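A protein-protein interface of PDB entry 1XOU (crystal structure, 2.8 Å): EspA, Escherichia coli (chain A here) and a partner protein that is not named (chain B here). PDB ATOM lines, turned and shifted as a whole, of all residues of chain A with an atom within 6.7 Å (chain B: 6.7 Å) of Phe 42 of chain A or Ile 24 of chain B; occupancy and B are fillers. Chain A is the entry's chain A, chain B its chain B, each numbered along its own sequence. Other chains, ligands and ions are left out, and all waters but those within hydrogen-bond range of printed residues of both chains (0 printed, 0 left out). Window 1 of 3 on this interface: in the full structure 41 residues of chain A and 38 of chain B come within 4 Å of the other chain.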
ATOM      1  N   ASN A  37       3.844  13.754  -8.161  1.00  0.00           N
ATOM      2  CA  ASN A  37       3.734  12.462  -7.492  1.00  0.00           C
ATOM      3  C   ASN A  37       4.312  11.305  -8.289  1.00  0.00           C
ATOM      4  O   ASN A  37       4.943  10.404  -7.732  1.00  0.00           O
ATOM      5  CB  ASN A  37       2.277  12.181  -7.146  1.00  0.00           C
ATOM      6  CG  ASN A  37       1.804  12.994  -5.961  1.00  0.00           C
ATOM      7  OD1 ASN A  37       2.161  12.705  -4.813  1.00  0.00           O
ATOM      8  ND2 ASN A  37       1.010  14.030  -6.229  1.00  0.00           N
ATOM      9  N   LYS A  38       4.081  11.335  -9.596  1.00  0.00           N
ATOM     10  CA  LYS A  38       4.579  10.304 -10.497  1.00  0.00           C
ATOM     11  C   LYS A  38       6.100  10.202 -10.343  1.00  0.00           C
ATOM     12  O   LYS A  38       6.638   9.150  -9.973  1.00  0.00           O
ATOM     13  CB  LYS A  38       4.226  10.671 -11.942  1.00  0.00           C
ATOM     14  CG  LYS A  38       3.340   9.668 -12.658  1.00  0.00           C
ATOM     15  CD  LYS A  38       1.885   9.805 -12.294  1.00  0.00           C
ATOM     16  CE  LYS A  38       1.077  10.401 -13.441  1.00  0.00           C
ATOM     17  NZ  LYS A  38       1.476  11.805 -13.741  1.00  0.00           N
ATOM     18  N   LEU A  39       6.777  11.314 -10.615  1.00  0.00           N
ATOM     19  CA  LEU A  39       8.225  11.397 -10.528  1.00  0.00           C
ATOM     20  C   LEU A  39       8.774  11.213  -9.118  1.00  0.00           C
ATOM     21  O   LEU A  39       9.869  10.668  -8.941  1.00  0.00           O
ATOM     22  CB  LEU A  39       8.703  12.735 -11.095  1.00  0.00           C
ATOM     23  CG  LEU A  39       8.779  12.850 -12.622  1.00  0.00           C
ATOM     24  CD1 LEU A  39       9.889  11.948 -13.163  1.00  0.00           C
ATOM     25  CD2 LEU A  39       7.442  12.447 -13.230  1.00  0.00           C
ATOM     26  N   GLY A  40       8.028  11.667  -8.118  1.00  0.00           N
ATOM     27  CA  GLY A  40       8.485  11.529  -6.751  1.00  0.00           C
ATOM     28  C   GLY A  40       8.523  10.074  -6.350  1.00  0.00           C
ATOM     29  O   GLY A  40       9.472   9.599  -5.718  1.00  0.00           O
ATOM     30  N   VAL A  41       7.479   9.347  -6.717  1.00  0.00           N
ATOM     31  CA  VAL A  41       7.430   7.941  -6.377  1.00  0.00           C
ATOM     32  C   VAL A  41       8.486   7.219  -7.207  1.00  0.00           C
ATOM     33  O   VAL A  41       9.225   6.373  -6.694  1.00  0.00           O
ATOM     34  CB  VAL A  41       6.002   7.360  -6.620  1.00  0.00           C
ATOM     35  CG1 VAL A  41       6.007   5.835  -6.532  1.00  0.00           C
ATOM     36  CG2 VAL A  41       5.045   7.931  -5.579  1.00  0.00           C
ATOM     37  N   PHE A  42       8.585   7.565  -8.485  1.00  0.00           N
ATOM     38  CA  PHE A  42       9.593   6.914  -9.307  1.00  0.00           C
ATOM     39  C   PHE A  42      11.007   7.183  -8.778  1.00  0.00           C
ATOM     40  O   PHE A  42      11.836   6.273  -8.657  1.00  0.00           O
ATOM     41  CB  PHE A  42       9.504   7.367 -10.761  1.00  0.00           C
ATOM     42  CG  PHE A  42      10.374   6.561 -11.676  1.00  0.00           C
ATOM     43  CD1 PHE A  42      11.505   7.117 -12.254  1.00  0.00           C
ATOM     44  CD2 PHE A  42      10.090   5.216 -11.907  1.00  0.00           C
ATOM     45  CE1 PHE A  42      12.349   6.349 -13.043  1.00  0.00           C
ATOM     46  CE2 PHE A  42      10.928   4.435 -12.694  1.00  0.00           C
ATOM     47  CZ  PHE A  42      12.061   4.999 -13.265  1.00  0.00           C
ATOM     48  N   GLN A  43      11.279   8.438  -8.457  1.00  0.00           N
ATOM     49  CA  GLN A  43      12.580   8.785  -7.947  1.00  0.00           C
ATOM     50  C   GLN A  43      12.875   8.052  -6.627  1.00  0.00           C
ATOM     51  O   GLN A  43      14.021   7.677  -6.341  1.00  0.00           O
ATOM     52  CB  GLN A  43      12.663  10.285  -7.743  1.00  0.00           C
ATOM     53  CG  GLN A  43      14.051  10.758  -7.388  1.00  0.00           C
ATOM     54  CD  GLN A  43      14.067  12.218  -7.062  1.00  0.00           C
ATOM     55  OE1 GLN A  43      15.128  12.806  -6.854  1.00  0.00           O
ATOM     56  NE2 GLN A  43      12.880  12.827  -7.012  1.00  0.00           N
ATOM     57  N   ALA A  44      11.842   7.848  -5.821  1.00  0.00           N
ATOM     58  CA  ALA A  44      12.030   7.148  -4.562  1.00  0.00           C
ATOM     59  C   ALA A  44      12.383   5.682  -4.846  1.00  0.00           C
ATOM     60  O   ALA A  44      13.214   5.093  -4.159  1.00  0.00           O
ATOM     61  CB  ALA A  44      10.765   7.253  -3.699  1.00  0.00           C
ATOM     62  N   ALA A  45      11.764   5.088  -5.860  1.00  0.00           N
ATOM     63  CA  ALA A  45      12.079   3.699  -6.197  1.00  0.00           C
ATOM     64  C   ALA A  45      13.566   3.597  -6.547  1.00  0.00           C
ATOM     65  O   ALA A  45      14.290   2.763  -5.995  1.00  0.00           O
ATOM     66  CB  ALA A  45      11.230   3.227  -7.370  1.00  0.00           C
ATOM     67  N   ILE A  46      14.009   4.470  -7.452  1.00  0.00           N
ATOM     68  CA  ILE A  46      15.398   4.511  -7.894  1.00  0.00           C
ATOM     69  C   ILE A  46      16.386   4.733  -6.754  1.00  0.00           C
ATOM     70  O   ILE A  46      17.384   4.017  -6.645  1.00  0.00           O
ATOM     71  CB  ILE A  46      15.621   5.621  -8.932  1.00  0.00           C
ATOM     72  CG1 ILE A  46      14.978   5.230 -10.260  1.00  0.00           C
ATOM     73  CG2 ILE A  46      17.105   5.840  -9.147  1.00  0.00           C
ATOM     74  CD1 ILE A  46      15.668   4.065 -10.952  1.00  0.00           C
ATOM     75  N   LEU A  47      16.126   5.735  -5.922  1.00  0.00           N
ATOM     76  CA  LEU A  47      17.005   6.025  -4.802  1.00  0.00           C
ATOM     77  C   LEU A  47      17.087   4.829  -3.854  1.00  0.00           C
ATOM     78  O   LEU A  47      18.165   4.498  -3.350  1.00  0.00           O
ATOM     79  CB  LEU A  47      16.507   7.270  -4.064  1.00  0.00           C
ATOM     80  CG  LEU A  47      17.190   8.634  -4.328  1.00  0.00           C
ATOM     81  CD1 LEU A  47      17.994   8.623  -5.637  1.00  0.00           C
ATOM     82  CD2 LEU A  47      16.114   9.727  -4.320  1.00  0.00           C
ATOM     83  N   LEU A 170      16.987  -3.050 -15.511  1.00  0.00           N
ATOM     84  CA  LEU A 170      17.310  -1.648 -15.290  1.00  0.00           C
ATOM     85  C   LEU A 170      17.351  -0.834 -16.574  1.00  0.00           C
ATOM     86  O   LEU A 170      16.963   0.325 -16.600  1.00  0.00           O
ATOM     87  CB  LEU A 170      18.655  -1.550 -14.588  1.00  0.00           C
ATOM     88  CG  LEU A 170      19.036  -0.196 -14.014  1.00  0.00           C
ATOM     89  CD1 LEU A 170      17.951   0.277 -13.038  1.00  0.00           C
ATOM     90  CD2 LEU A 170      20.397  -0.337 -13.319  1.00  0.00           C
ATOM     91  N   THR A 171      17.834  -1.434 -17.646  1.00  0.00           N
ATOM     92  CA  THR A 171      17.898  -0.731 -18.919  1.00  0.00           C
ATOM     93  C   THR A 171      16.513  -0.660 -19.570  1.00  0.00           C
ATOM     94  O   THR A 171      16.203   0.271 -20.315  1.00  0.00           O
ATOM     95  CB  THR A 171      18.884  -1.432 -19.855  1.00  0.00           C
ATOM     96  OG1 THR A 171      20.196  -1.364 -19.274  1.00  0.00           O
ATOM     97  CG2 THR A 171      18.889  -0.770 -21.229  1.00  0.00           C
ATOM     98  N   ALA A 173      13.732  -0.359 -17.876  1.00  0.00           N
ATOM     99  CA  ALA A 173      13.107   0.729 -17.138  1.00  0.00           C
ATOM    100  C   ALA A 173      13.548   2.048 -17.734  1.00  0.00           C
ATOM    101  O   ALA A 173      12.745   2.956 -17.918  1.00  0.00           O
ATOM    102  CB  ALA A 173      13.519   0.667 -15.674  1.00  0.00           C
ATOM    103  N   ARG A 174      14.837   2.147 -18.043  1.00  0.00           N
ATOM    104  CA  ARG A 174      15.389   3.373 -18.615  1.00  0.00           C
ATOM    105  C   ARG A 174      14.748   3.684 -19.952  1.00  0.00           C
ATOM    106  O   ARG A 174      14.405   4.830 -20.218  1.00  0.00           O
ATOM    107  CB  ARG A 174      16.906   3.257 -18.782  1.00  0.00           C
ATOM    108  CG  ARG A 174      17.627   4.604 -18.815  1.00  0.00           C
ATOM    109  CD  ARG A 174      18.201   4.901 -20.181  1.00  0.00           C
ATOM    110  NE  ARG A 174      19.126   3.848 -20.584  1.00  0.00           N
ATOM    111  CZ  ARG A 174      19.130   3.278 -21.786  1.00  0.00           C
ATOM    112  NH1 ARG A 174      20.007   2.323 -22.062  1.00  0.00           N
ATOM    113  NH2 ARG A 174      18.256   3.659 -22.710  1.00  0.00           N
ATOM    114  N   SER A 175      14.582   2.662 -20.787  1.00  0.00           N
ATOM    115  CA  SER A 175      13.959   2.827 -22.102  1.00  0.00           C
ATOM    116  C   SER A 175      12.532   3.340 -21.974  1.00  0.00           C
ATOM    117  O   SER A 175      12.107   4.210 -22.739  1.00  0.00           O
ATOM    118  CB  SER A 175      13.931   1.502 -22.844  1.00  0.00           C
ATOM    119  OG  SER A 175      15.241   0.993 -22.981  1.00  0.00           O
ATOM    120  N   MET A 177      11.243   5.086 -19.456  1.00  0.00           N
ATOM    121  CA  MET A 177      11.244   6.479 -19.042  1.00  0.00           C
ATOM    122  C   MET A 177      11.584   7.397 -20.196  1.00  0.00           C
ATOM    123  O   MET A 177      11.181   8.556 -20.220  1.00  0.00           O
ATOM    124  CB  MET A 177      12.207   6.703 -17.873  1.00  0.00           C
ATOM    125  CG  MET A 177      11.676   6.145 -16.555  1.00  0.00           C
ATOM    126  SD  MET A 177       9.782   6.595 -16.259  1.00  0.00           S
ATOM    127  CE  MET A 177      10.027   8.405 -15.607  1.00  0.00           C
ATOM    128  N   SER B  19      25.875   3.325 -14.621  1.00  0.00           N
ATOM    129  CA  SER B  19      25.569   4.256 -15.702  1.00  0.00           C
ATOM    130  C   SER B  19      24.061   4.343 -15.874  1.00  0.00           C
ATOM    131  O   SER B  19      23.502   5.426 -16.044  1.00  0.00           O
ATOM    132  CB  SER B  19      26.189   3.782 -17.016  1.00  0.00           C
ATOM    133  OG  SER B  19      27.598   3.779 -16.946  1.00  0.00           O
ATOM    134  N   GLU B  20      23.413   3.185 -15.832  1.00  0.00           N
ATOM    135  CA  GLU B  20      21.974   3.118 -15.974  1.00  0.00           C
ATOM    136  C   GLU B  20      21.306   3.889 -14.848  1.00  0.00           C
ATOM    137  O   GLU B  20      20.231   4.468 -15.045  1.00  0.00           O
ATOM    138  CB  GLU B  20      21.518   1.661 -15.983  1.00  0.00           C
ATOM    139  CG  GLU B  20      20.647   1.330 -17.175  1.00  0.00           C
ATOM    140  CD  GLU B  20      21.263   1.798 -18.484  1.00  0.00           C
ATOM    141  OE1 GLU B  20      20.613   1.664 -19.547  1.00  0.00           O
ATOM    142  OE2 GLU B  20      22.408   2.301 -18.452  1.00  0.00           O
ATOM    143  N   ILE B  21      21.940   3.905 -13.673  1.00  0.00           N
ATOM    144  CA  ILE B  21      21.386   4.643 -12.541  1.00  0.00           C
ATOM    145  C   ILE B  21      21.506   6.149 -12.803  1.00  0.00           C
ATOM    146  O   ILE B  21      20.538   6.895 -12.670  1.00  0.00           O
ATOM    147  CB  ILE B  21      22.115   4.348 -11.216  1.00  0.00           C
ATOM    148  CG1 ILE B  21      22.376   2.847 -11.056  1.00  0.00           C
ATOM    149  CG2 ILE B  21      21.290   4.877 -10.061  1.00  0.00           C
ATOM    150  CD1 ILE B  21      21.162   2.001 -11.011  1.00  0.00           C
ATOM    151  N   GLU B  22      22.693   6.594 -13.188  1.00  0.00           N
ATOM    152  CA  GLU B  22      22.889   8.009 -13.449  1.00  0.00           C
ATOM    153  C   GLU B  22      22.019   8.476 -14.607  1.00  0.00           C
ATOM    154  O   GLU B  22      21.470   9.577 -14.566  1.00  0.00           O
ATOM    155  CB  GLU B  22      24.357   8.294 -13.755  1.00  0.00           C
ATOM    156  CG  GLU B  22      25.325   7.880 -12.648  1.00  0.00           C
ATOM    157  CD  GLU B  22      25.010   8.525 -11.304  1.00  0.00           C
ATOM    158  OE1 GLU B  22      24.859   9.767 -11.259  1.00  0.00           O
ATOM    159  OE2 GLU B  22      24.922   7.790 -10.293  1.00  0.00           O
ATOM    160  N   ALA B  23      21.896   7.639 -15.635  1.00  0.00           N
ATOM    161  CA  ALA B  23      21.085   7.967 -16.811  1.00  0.00           C
ATOM    162  C   ALA B  23      19.652   8.234 -16.375  1.00  0.00           C
ATOM    163  O   ALA B  23      19.047   9.231 -16.776  1.00  0.00           O
ATOM    164  CB  ALA B  23      21.109   6.820 -17.802  1.00  0.00           C
ATOM    165  N   ILE B  24      19.127   7.336 -15.541  1.00  0.00           N
ATOM    166  CA  ILE B  24      17.772   7.446 -15.034  1.00  0.00           C
ATOM    167  C   ILE B  24      17.637   8.687 -14.175  1.00  0.00           C
ATOM    168  O   ILE B  24      16.694   9.467 -14.349  1.00  0.00           O
ATOM    169  CB  ILE B  24      17.397   6.175 -14.241  1.00  0.00           C
ATOM    170  CG1 ILE B  24      17.365   4.985 -15.216  1.00  0.00           C
ATOM    171  CG2 ILE B  24      16.048   6.357 -13.523  1.00  0.00           C
ATOM    172  CD1 ILE B  24      17.229   3.640 -14.570  1.00  0.00           C
ATOM    173  N   LYS B  25      18.583   8.884 -13.260  1.00  0.00           N
ATOM    174  CA  LYS B  25      18.554  10.062 -12.402  1.00  0.00           C
ATOM    175  C   LYS B  25      18.539  11.327 -13.272  1.00  0.00           C
ATOM    176  O   LYS B  25      17.874  12.321 -12.938  1.00  0.00           O
ATOM    177  CB  LYS B  25      19.761  10.062 -11.461  1.00  0.00           C
ATOM    178  CG  LYS B  25      19.754   8.896 -10.477  1.00  0.00           C
ATOM    179  CD  LYS B  25      20.969   8.890  -9.535  1.00  0.00           C
ATOM    180  CE  LYS B  25      20.779   9.860  -8.376  1.00  0.00           C
ATOM    181  NZ  LYS B  25      21.773   9.654  -7.258  1.00  0.00           N
ATOM    182  N   LYS B  26      19.253  11.283 -14.394  1.00  0.00           N
ATOM    183  CA  LYS B  26      19.287  12.419 -15.308  1.00  0.00           C
ATOM    184  C   LYS B  26      17.940  12.576 -15.999  1.00  0.00           C
ATOM    185  O   LYS B  26      17.410  13.685 -16.057  1.00  0.00           O
ATOM    186  CB  LYS B  26      20.373  12.244 -16.368  1.00  0.00           C
ATOM    187  CG  LYS B  26      21.809  12.344 -15.861  1.00  0.00           C
ATOM    188  CD  LYS B  26      22.781  12.005 -16.989  1.00  0.00           C
ATOM    189  CE  LYS B  26      24.233  12.249 -16.609  1.00  0.00           C
ATOM    190  NZ  LYS B  26      25.108  12.191 -17.823  1.00  0.00           N
ATOM    191  N   ILE B  27      17.397  11.479 -16.531  1.00  0.00           N
ATOM    192  CA  ILE B  27      16.099  11.510 -17.204  1.00  0.00           C
ATOM    193  C   ILE B  27      15.055  12.131 -16.267  1.00  0.00           C
ATOM    194  O   ILE B  27      14.197  12.921 -16.682  1.00  0.00           O
ATOM    195  CB  ILE B  27      15.582  10.097 -17.538  1.00  0.00           C
ATOM    196  CG1 ILE B  27      16.622   9.306 -18.334  1.00  0.00           C
ATOM    197  CG2 ILE B  27      14.271  10.203 -18.321  1.00  0.00           C
ATOM    198  CD1 ILE B  27      16.866   9.817 -19.730  1.00  0.00           C
ATOM    199  N   ILE B  28      15.119  11.748 -14.998  1.00  0.00           N
ATOM    200  CA  ILE B  28      14.177  12.263 -14.026  1.00  0.00           C
ATOM    201  C   ILE B  28      14.332  13.769 -13.912  1.00  0.00           C
ATOM    202  O   ILE B  28      13.347  14.497 -13.839  1.00  0.00           O
ATOM    203  CB  ILE B  28      14.391  11.592 -12.654  1.00  0.00           C
ATOM    204  CG1 ILE B  28      13.824  10.174 -12.690  1.00  0.00           C
ATOM    205  CG2 ILE B  28      13.756  12.418 -11.547  1.00  0.00           C
ATOM    206  CD1 ILE B  28      14.145   9.377 -11.466  1.00  0.00           C
ATOM    207  N   ALA B  29      15.573  14.239 -13.902  1.00  0.00           N
ATOM    208  CA  ALA B  29      15.829  15.674 -13.814  1.00  0.00           C
ATOM    209  C   ALA B  29      15.269  16.396 -15.049  1.00  0.00           C
ATOM    210  O   ALA B  29      14.612  17.421 -14.917  1.00  0.00           O
ATOM    211  CB  ALA B  29      17.317  15.925 -13.677  1.00  0.00           C
ATOM    212  N   TYR B  71       4.866   4.520 -17.766  1.00  0.00           N
ATOM    213  CA  TYR B  71       5.254   4.889 -16.410  1.00  0.00           C
ATOM    214  C   TYR B  71       5.142   3.709 -15.430  1.00  0.00           C
ATOM    215  O   TYR B  71       6.081   3.407 -14.698  1.00  0.00           O
ATOM    216  CB  TYR B  71       4.387   6.056 -15.928  1.00  0.00           C
ATOM    217  CG  TYR B  71       4.594   6.364 -14.473  1.00  0.00           C
ATOM    218  CD1 TYR B  71       5.669   7.145 -14.056  1.00  0.00           C
ATOM    219  CD2 TYR B  71       3.776   5.785 -13.493  1.00  0.00           C
ATOM    220  CE1 TYR B  71       5.932   7.339 -12.701  1.00  0.00           C
ATOM    221  CE2 TYR B  71       4.030   5.973 -12.134  1.00  0.00           C
ATOM    222  CZ  TYR B  71       5.112   6.747 -11.749  1.00  0.00           C
ATOM    223  OH  TYR B  71       5.395   6.908 -10.420  1.00  0.00           O
ATOM    224  N   SER B  73       5.095   0.647 -16.110  1.00  0.00           N
ATOM    225  CA  SER B  73       6.019  -0.374 -16.545  1.00  0.00           C
ATOM    226  C   SER B  73       7.389  -0.150 -15.907  1.00  0.00           C
ATOM    227  O   SER B  73       7.926  -1.031 -15.236  1.00  0.00           O
ATOM    228  CB  SER B  73       6.132  -0.337 -18.064  1.00  0.00           C
ATOM    229  OG  SER B  73       6.950  -1.389 -18.526  1.00  0.00           O
ATOM    230  N   ALA B  74       7.946   1.041 -16.111  1.00  0.00           N
ATOM    231  CA  ALA B  74       9.249   1.386 -15.551  1.00  0.00           C
ATOM    232  C   ALA B  74       9.257   1.259 -14.031  1.00  0.00           C
ATOM    233  O   ALA B  74      10.180   0.681 -13.456  1.00  0.00           O
ATOM    234  CB  ALA B  74       9.631   2.811 -15.949  1.00  0.00           C
ATOM    235  N   LEU B  75       8.226   1.796 -13.385  1.00  0.00           N
ATOM    236  CA  LEU B  75       8.132   1.761 -11.928  1.00  0.00           C
ATOM    237  C   LEU B  75       8.100   0.349 -11.361  1.00  0.00           C
ATOM    238  O   LEU B  75       8.741   0.078 -10.355  1.00  0.00           O
ATOM    239  CB  LEU B  75       6.891   2.534 -11.469  1.00  0.00           C
ATOM    240  CG  LEU B  75       6.731   3.023 -10.020  1.00  0.00           C
ATOM    241  CD1 LEU B  75       5.563   2.310  -9.394  1.00  0.00           C
ATOM    242  CD2 LEU B  75       8.008   2.821  -9.215  1.00  0.00           C
ATOM    243  N   SER B  76       7.377  -0.557 -12.012  1.00  0.00           N
ATOM    244  CA  SER B  76       7.279  -1.933 -11.525  1.00  0.00           C
ATOM    245  C   SER B  76       8.565  -2.710 -11.735  1.00  0.00           C
ATOM    246  O   SER B  76       8.853  -3.656 -11.006  1.00  0.00           O
ATOM    247  CB  SER B  76       6.129  -2.655 -12.208  1.00  0.00           C
ATOM    248  OG  SER B  76       6.303  -2.602 -13.605  1.00  0.00           O
ATOM    249  N   ILE B  78      11.501  -1.341 -11.458  1.00  0.00           N
ATOM    250  CA  ILE B  78      12.364  -0.888 -10.385  1.00  0.00           C
ATOM    251  C   ILE B  78      11.922  -1.552  -9.096  1.00  0.00           C
ATOM    252  O   ILE B  78      12.750  -1.917  -8.261  1.00  0.00           O
ATOM    253  CB  ILE B  78      12.323   0.655 -10.191  1.00  0.00           C
ATOM    254  CG1 ILE B  78      12.876   1.357 -11.434  1.00  0.00           C
ATOM    255  CG2 ILE B  78      13.186   1.059  -8.975  1.00  0.00           C
ATOM    256  CD1 ILE B  78      14.317   0.954 -11.776  1.00  0.00           C
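Hydrophobic or aromatic side chains of chain B within 4 Å of the printed part of chain A: Ile 21, Ile 24, Ile 27, Ile 28, Tyr 71, Ala 74, Leu 75 and Ile 78.
Printed residues of chain A that touch a printed residue of chain B: Lys 38, Val 41, Phe 42, Gln 43, Ala 45, Ile 46, Leu 170, Thr 171, Ala 173, Arg 174 and Met 177.
Printed residues of chain B within 4 Å of Phe 42 of chain A: Ile 24 (3.7 Å), Ile 28 (3.6 Å), Tyr 71 (3.8 Å), Ala 74 (3.8 Å), Leu 75 (3.8 Å) and Ile 78 (3.9 Å).
Of chain A, only Phe 42, Ile 46, Leu 170 and Arg 174 come within 4 Å of Ile 24 of chain B.
Of the printed residues of chain A, Ala 74 of chain B touches Phe 42, Ala 173 and Met 177.
Of the printed residues of chain A, Glu 20 of chain B touches Leu 170, Thr 171 and Arg 174.
Printed residues of chain A within 4 Å of Leu 75 of chain B: Phe 42 and Ala 45.
Printed residues of chain B within 4 Å of Gln 43 of chain A: Ile 28.
Of the printed residues of chain A, Tyr 71 of chain B touches Lys 38 (2.6 Å), Val 41 (3.9 Å) and Phe 42 (3.8 Å).
Ala 44 of chain A touches none of the printed residues of chain B.
The nearest residue of chain A that does not touch Ile 24 of chain B is Ala 173 of chain A (4.9 Å).
The nearest printed residue of chain B that does not touch Gln 43 of chain A is Tyr 71 of chain B (6.4 Å).
The backbone carbonyl oxygen (O) of Thr 171 of chain A sits at hydrogen-bond distance from the side-chain hydroxyl (OG) of Ser 175 of chain A (2.9 Å).
Among the printed residues, pairs that only touch across the chains: Val 41 of chain A with Tyr 71 of chain B (3.9 Å), Phe 42 of chain A with Ile 24 of chain B (3.7 Å), Phe 42 of chain A with Ile 28 of chain B (3.6 Å), Phe 42 of chain A with Tyr 71 of chain B (3.8 Å), Phe 42 of chain A with Ala 74 of chain B (3.8 Å), Phe 42 of chain A with Leu 75 of chain B (3.8 Å), Phe 42 of chain A with Ile 78 of chain B (3.9 Å), Gln 43 of chain A with Ile 28 of chain B (3.9 Å), Ala 45 of chain A with Leu 75 of chain B (3.7 Å), Ala 45 of chain A with Ile 78 of chain B (3.3 Å), Ile 46 of chain A with Ile 24 of chain B (3.5 Å), Ile 46 of chain A with Ile 78 of chain B (3.5 Å), Leu 170 of chain A with Glu 20 of chain B (3.5 Å), Leu 170 of chain A with Ile 21 of chain B (3.4 Å), Leu 170 of chain A with Ile 24 of chain B (3.8 Å), Leu 170 of chain A with Ile 78 of chain B (3.9 Å), Ala 173 of chain A with Ala 74 of chain B (3.7 Å), Ala 173 of chain A with Ile 78 of chain B (3.99 Å), Arg 174 of chain A with Ile 24 of chain B (3.6 Å), Met 177 of chain A with Ile 27 of chain B (3.98 Å) and Met 177 of chain A with Ala 74 of chain B (3.8 Å).
O of Lys 38 of chain A lies within hydrogen-bond range of OH of Tyr 71 of chain B (2.6 Å).
The side-chain carboxylate of Glu 20 of chain B is in hydrogen-bond range of the side-chain hydroxyl of Thr 171 of chain A.
NH1 of Arg 174 of chain A lies within salt-bridge range of OE1 of Glu 20 of chain B, 2.7 Å away.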
